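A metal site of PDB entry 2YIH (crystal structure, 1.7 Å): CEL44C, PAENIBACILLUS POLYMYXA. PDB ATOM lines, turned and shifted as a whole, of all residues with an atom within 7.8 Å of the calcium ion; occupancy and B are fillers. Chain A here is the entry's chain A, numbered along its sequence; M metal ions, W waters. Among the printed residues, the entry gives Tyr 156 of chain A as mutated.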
ATOM      1  N   ASN A  54      14.752 -18.723  -9.367  1.00  0.00           N
ATOM      2  CA  ASN A  54      13.765 -19.794  -9.210  1.00  0.00           C
ATOM      3  C   ASN A  54      13.554 -19.970  -7.710  1.00  0.00           C
ATOM      4  O   ASN A  54      14.449 -20.422  -7.000  1.00  0.00           O
ATOM      5  CB  ASN A  54      14.373 -21.066  -9.795  1.00  0.00           C
ATOM      6  CG  ASN A  54      13.476 -22.287  -9.637  1.00  0.00           C
ATOM      7  OD1 ASN A  54      12.545 -22.277  -8.830  1.00  0.00           O
ATOM      8  ND2 ASN A  54      13.739 -23.342 -10.425  1.00  0.00           N
ATOM      9  N   TRP A  55      12.391 -19.582  -7.190  1.00  0.00           N
ATOM     10  CA  TRP A  55      12.177 -19.660  -5.738  1.00  0.00           C
ATOM     11  C   TRP A  55      12.224 -21.075  -5.180  1.00  0.00           C
ATOM     12  O   TRP A  55      12.479 -21.287  -3.975  1.00  0.00           O
ATOM     13  CB  TRP A  55      10.867 -18.971  -5.357  1.00  0.00           C
ATOM     14  CG  TRP A  55       9.604 -19.803  -5.589  1.00  0.00           C
ATOM     15  CD1 TRP A  55       8.900 -19.899  -6.766  1.00  0.00           C
ATOM     16  CD2 TRP A  55       8.839 -20.512  -4.589  1.00  0.00           C
ATOM     17  NE1 TRP A  55       7.770 -20.687  -6.563  1.00  0.00           N
ATOM     18  CE2 TRP A  55       7.716 -21.086  -5.244  1.00  0.00           C
ATOM     19  CE3 TRP A  55       8.993 -20.746  -3.205  1.00  0.00           C
ATOM     20  CZ2 TRP A  55       6.766 -21.854  -4.587  1.00  0.00           C
ATOM     21  CZ3 TRP A  55       8.043 -21.532  -2.535  1.00  0.00           C
ATOM     22  CH2 TRP A  55       6.930 -22.060  -3.232  1.00  0.00           C
ATOM     23  N   GLU A  56      11.873 -22.063  -6.021  1.00  0.00           N
ATOM     24  CA  GLU A  56      11.781 -23.436  -5.535  1.00  0.00           C
ATOM     25  C   GLU A  56      13.123 -23.981  -5.103  1.00  0.00           C
ATOM     26  O   GLU A  56      13.193 -24.736  -4.119  1.00  0.00           O
ATOM     27  CB  GLU A  56      11.146 -24.380  -6.577  1.00  0.00           C
ATOM     28  CG  GLU A  56       9.768 -23.901  -7.076  1.00  0.00           C
ATOM     29  CD  GLU A  56       9.175 -24.868  -8.076  1.00  0.00           C
ATOM     30  OE1 GLU A  56       9.941 -25.668  -8.680  1.00  0.00           O
ATOM     31  OE2 GLU A  56       7.953 -24.856  -8.250  1.00  0.00           O
ATOM     32  N   ASN A 136      13.251 -23.691 -16.364  1.00  0.00           N
ATOM     33  CA  ASN A 136      11.855 -23.999 -16.075  1.00  0.00           C
ATOM     34  C   ASN A 136      10.997 -22.823 -16.511  1.00  0.00           C
ATOM     35  O   ASN A 136      11.455 -21.674 -16.469  1.00  0.00           O
ATOM     36  CB  ASN A 136      11.657 -24.226 -14.569  1.00  0.00           C
ATOM     37  CG  ASN A 136      12.330 -25.492 -14.076  1.00  0.00           C
ATOM     38  OD1 ASN A 136      12.423 -26.469 -14.816  1.00  0.00           O
ATOM     39  ND2 ASN A 136      12.763 -25.503 -12.809  1.00  0.00           N
ATOM     40  N   GLN A 137       9.772 -23.112 -16.929  1.00  0.00           N
ATOM     41  CA  GLN A 137       8.860 -22.071 -17.417  1.00  0.00           C
ATOM     42  C   GLN A 137       8.175 -21.390 -16.243  1.00  0.00           C
ATOM     43  O   GLN A 137       7.728 -22.051 -15.288  1.00  0.00           O
ATOM     44  CB  GLN A 137       7.788 -22.691 -18.313  1.00  0.00           C
ATOM     45  CG  GLN A 137       8.291 -23.288 -19.562  1.00  0.00           C
ATOM     46  CD  GLN A 137       7.149 -23.796 -20.444  1.00  0.00           C
ATOM     47  OE1 GLN A 137       6.019 -23.260 -20.424  1.00  0.00           O
ATOM     48  NE2 GLN A 137       7.424 -24.848 -21.214  1.00  0.00           N
ATOM     49  N   GLN A 147       1.002 -25.464  -2.988  1.00  0.00           N
ATOM     50  CA  GLN A 147       1.825 -26.274  -2.116  1.00  0.00           C
ATOM     51  C   GLN A 147       2.812 -25.342  -1.428  1.00  0.00           C
ATOM     52  O   GLN A 147       3.472 -24.546  -2.082  1.00  0.00           O
ATOM     53  CB  GLN A 147       2.582 -27.341  -2.951  1.00  0.00           C
ATOM     54  CG  GLN A 147       1.661 -28.268  -3.786  1.00  0.00           C
ATOM     55  CD  GLN A 147       2.418 -29.043  -4.888  1.00  0.00           C
ATOM     56  OE1 GLN A 147       2.565 -28.583  -6.046  1.00  0.00           O
ATOM     57  NE2 GLN A 147       2.941 -30.214  -4.514  1.00  0.00           N
ATOM     58  N   PRO A 150       6.855 -26.764  -2.919  1.00  0.00           N
ATOM     59  CA  PRO A 150       6.486 -26.856  -4.334  1.00  0.00           C
ATOM     60  C   PRO A 150       7.047 -28.085  -5.021  1.00  0.00           C
ATOM     61  O   PRO A 150       7.988 -28.722  -4.519  1.00  0.00           O
ATOM     62  CB  PRO A 150       7.103 -25.585  -4.946  1.00  0.00           C
ATOM     63  CG  PRO A 150       8.321 -25.305  -4.039  1.00  0.00           C
ATOM     64  CD  PRO A 150       7.803 -25.651  -2.658  1.00  0.00           C
ATOM     65  N   ASP A 151       6.469 -28.422  -6.176  1.00  0.00           N
ATOM     66  CA  ASP A 151       6.898 -29.598  -6.927  1.00  0.00           C
ATOM     67  C   ASP A 151       8.241 -29.293  -7.565  1.00  0.00           C
ATOM     68  O   ASP A 151       8.324 -28.464  -8.475  1.00  0.00           O
ATOM     69  CB  ASP A 151       5.845 -29.911  -7.991  1.00  0.00           C
ATOM     70  CG  ASP A 151       6.047 -31.267  -8.639  1.00  0.00           C
ATOM     71  OD1 ASP A 151       7.200 -31.746  -8.718  1.00  0.00           O
ATOM     72  OD2 ASP A 151       5.029 -31.822  -9.106  1.00  0.00           O
ATOM     73  N   LEU A 152       9.287 -30.005  -7.140  1.00  0.00           N
ATOM     74  CA  LEU A 152      10.629 -29.800  -7.688  1.00  0.00           C
ATOM     75  C   LEU A 152      10.896 -30.575  -8.982  1.00  0.00           C
ATOM     76  O   LEU A 152      11.932 -30.392  -9.639  1.00  0.00           O
ATOM     77  CB  LEU A 152      11.680 -30.172  -6.642  1.00  0.00           C
ATOM     78  CG  LEU A 152      11.574 -29.442  -5.288  1.00  0.00           C
ATOM     79  CD1 LEU A 152      12.663 -29.964  -4.341  1.00  0.00           C
ATOM     80  CD2 LEU A 152      11.711 -27.914  -5.491  1.00  0.00           C
ATOM     81  N   ASN A 153       9.965 -31.461  -9.352  1.00  0.00           N
ATOM     82  CA  ASN A 153      10.209 -32.426 -10.416  1.00  0.00           C
ATOM     83  C   ASN A 153       9.525 -32.070 -11.734  1.00  0.00           C
ATOM     84  O   ASN A 153       9.712 -32.771 -12.756  1.00  0.00           O
ATOM     85  CB  ASN A 153       9.795 -33.833  -9.983  1.00  0.00           C
ATOM     86  CG  ASN A 153      10.667 -34.346  -8.879  1.00  0.00           C
ATOM     87  OD1 ASN A 153      10.177 -34.923  -7.916  1.00  0.00           O
ATOM     88  ND2 ASN A 153      11.954 -34.066  -8.960  1.00  0.00           N
ATOM     89  N   ASP A 154       8.767 -30.977 -11.727  1.00  0.00           N
ATOM     90  CA  ASP A 154       8.107 -30.566 -12.962  1.00  0.00           C
ATOM     91  C   ASP A 154       8.896 -29.456 -13.641  1.00  0.00           C
ATOM     92  O   ASP A 154       9.984 -29.085 -13.186  1.00  0.00           O
ATOM     93  CB  ASP A 154       6.625 -30.172 -12.705  1.00  0.00           C
ATOM     94  CG  ASP A 154       6.471 -28.923 -11.862  1.00  0.00           C
ATOM     95  OD1 ASP A 154       7.511 -28.289 -11.555  1.00  0.00           O
ATOM     96  OD2 ASP A 154       5.309 -28.560 -11.560  1.00  0.00           O
ATOM     97  N   ASN A 155       8.359 -28.922 -14.731  1.00  0.00           N
ATOM     98  CA  ASN A 155       9.094 -27.922 -15.511  1.00  0.00           C
ATOM     99  C   ASN A 155       8.613 -26.495 -15.277  1.00  0.00           C
ATOM    100  O   ASN A 155       8.830 -25.624 -16.125  1.00  0.00           O
ATOM    101  CB  ASN A 155       8.961 -28.249 -17.010  1.00  0.00           C
ATOM    102  CG  ASN A 155      10.041 -27.601 -17.859  1.00  0.00           C
ATOM    103  OD1 ASN A 155      11.216 -27.537 -17.480  1.00  0.00           O
ATOM    104  ND2 ASN A 155       9.626 -27.062 -19.020  1.00  0.00           N
ATOM    105  N   TYR A 156       7.961 -26.264 -14.127  1.00  0.00           N
ATOM    106  CA  TYR A 156       7.235 -25.003 -13.923  1.00  0.00           C
ATOM    107  C   TYR A 156       7.630 -24.363 -12.622  1.00  0.00           C
ATOM    108  O   TYR A 156       7.882 -25.075 -11.647  1.00  0.00           O
ATOM    109  CB  TYR A 156       5.732 -25.267 -13.842  1.00  0.00           C
ATOM    110  CG  TYR A 156       5.184 -25.832 -15.137  1.00  0.00           C
ATOM    111  CD1 TYR A 156       5.121 -25.030 -16.265  1.00  0.00           C
ATOM    112  CD2 TYR A 156       4.834 -27.191 -15.233  1.00  0.00           C
ATOM    113  CE1 TYR A 156       4.666 -25.562 -17.476  1.00  0.00           C
ATOM    114  CE2 TYR A 156       4.408 -27.721 -16.414  1.00  0.00           C
ATOM    115  CZ  TYR A 156       4.309 -26.931 -17.526  1.00  0.00           C
ATOM    116  OH  TYR A 156       3.878 -27.451 -18.717  1.00  0.00           O
ATOM    117  N   VAL A 157       7.507 -23.050 -12.576  1.00  0.00           N
ATOM    118  CA  VAL A 157       7.532 -22.344 -11.293  1.00  0.00           C
ATOM    119  C   VAL A 157       6.313 -21.429 -11.323  1.00  0.00           C
ATOM    120  O   VAL A 157       6.067 -20.802 -12.341  1.00  0.00           O
ATOM    121  CB  VAL A 157       8.849 -21.556 -11.149  1.00  0.00           C
ATOM    122  CG1 VAL A 157       8.795 -20.649  -9.998  1.00  0.00           C
ATOM    123  CG2 VAL A 157      10.029 -22.555 -11.007  1.00  0.00           C
ATOM    124  N   TYR A 158       5.513 -21.428 -10.265  1.00  0.00           N
ATOM    125  CA  TYR A 158       4.254 -20.683 -10.285  1.00  0.00           C
ATOM    126  C   TYR A 158       4.399 -19.449  -9.436  1.00  0.00           C
ATOM    127  O   TYR A 158       4.684 -19.554  -8.254  1.00  0.00           O
ATOM    128  CB  TYR A 158       3.152 -21.558  -9.694  1.00  0.00           C
ATOM    129  CG  TYR A 158       2.839 -22.771 -10.561  1.00  0.00           C
ATOM    130  CD1 TYR A 158       2.181 -22.604 -11.774  1.00  0.00           C
ATOM    131  CD2 TYR A 158       3.275 -24.060 -10.190  1.00  0.00           C
ATOM    132  CE1 TYR A 158       1.873 -23.699 -12.591  1.00  0.00           C
ATOM    133  CE2 TYR A 158       2.996 -25.173 -11.018  1.00  0.00           C
ATOM    134  CZ  TYR A 158       2.301 -24.976 -12.206  1.00  0.00           C
ATOM    135  OH  TYR A 158       1.992 -26.064 -12.986  1.00  0.00           O
ATOM    136  N   GLU A 161       1.875 -19.037  -6.452  1.00  0.00           N
ATOM    137  CA  GLU A 161       2.221 -20.000  -5.410  1.00  0.00           C
ATOM    138  C   GLU A 161       3.308 -19.450  -4.495  1.00  0.00           C
ATOM    139  O   GLU A 161       3.280 -19.622  -3.279  1.00  0.00           O
ATOM    140  CB  GLU A 161       2.667 -21.322  -6.052  1.00  0.00           C
ATOM    141  CG  GLU A 161       2.893 -22.421  -5.004  1.00  0.00           C
ATOM    142  CD  GLU A 161       2.985 -23.792  -5.637  1.00  0.00           C
ATOM    143  OE1 GLU A 161       3.885 -23.993  -6.469  1.00  0.00           O
ATOM    144  OE2 GLU A 161       2.119 -24.635  -5.348  1.00  0.00           O
HETATM  145 CA    CA M   1       8.160 -26.673  -9.948  1.00  0.00          CA
HETATM  146  O   HOH W   1      10.194 -27.414 -10.949  1.00  0.00           O
HETATM  147  O   HOH W   2       5.722 -26.689  -9.635  1.00  0.00           O
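Four residues have an atom within 4 Å of the calcium ion: Glu 56, Asp 151, Asp 154 and Tyr 156.
The nearest printed residue that does not touch the calcium ion is Leu 152 (4.5 Å).
The side-chain carboxylate (OD1) of Asp 151 lies within hydrogen-bond range of the backbone NH (N) of Asn 153 (2.9 Å).
The backbone NH (N) of Glu 56 sits at hydrogen-bond distance from the side-chain amide oxygen (OD1) of Asn 54.
The calcium ion is bound by O of Asp 151 (2.3 Å), O of Tyr 156 (2.3 Å), OD1 of Asp 154 (2.4 Å), water W1 (2.4 Å), OE1 of Glu 56 (2.4 Å), water W2 (2.5 Å) and OE2 of Glu 56 (2.5 Å).
The calcium ion has seven donor atoms within binding distance.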
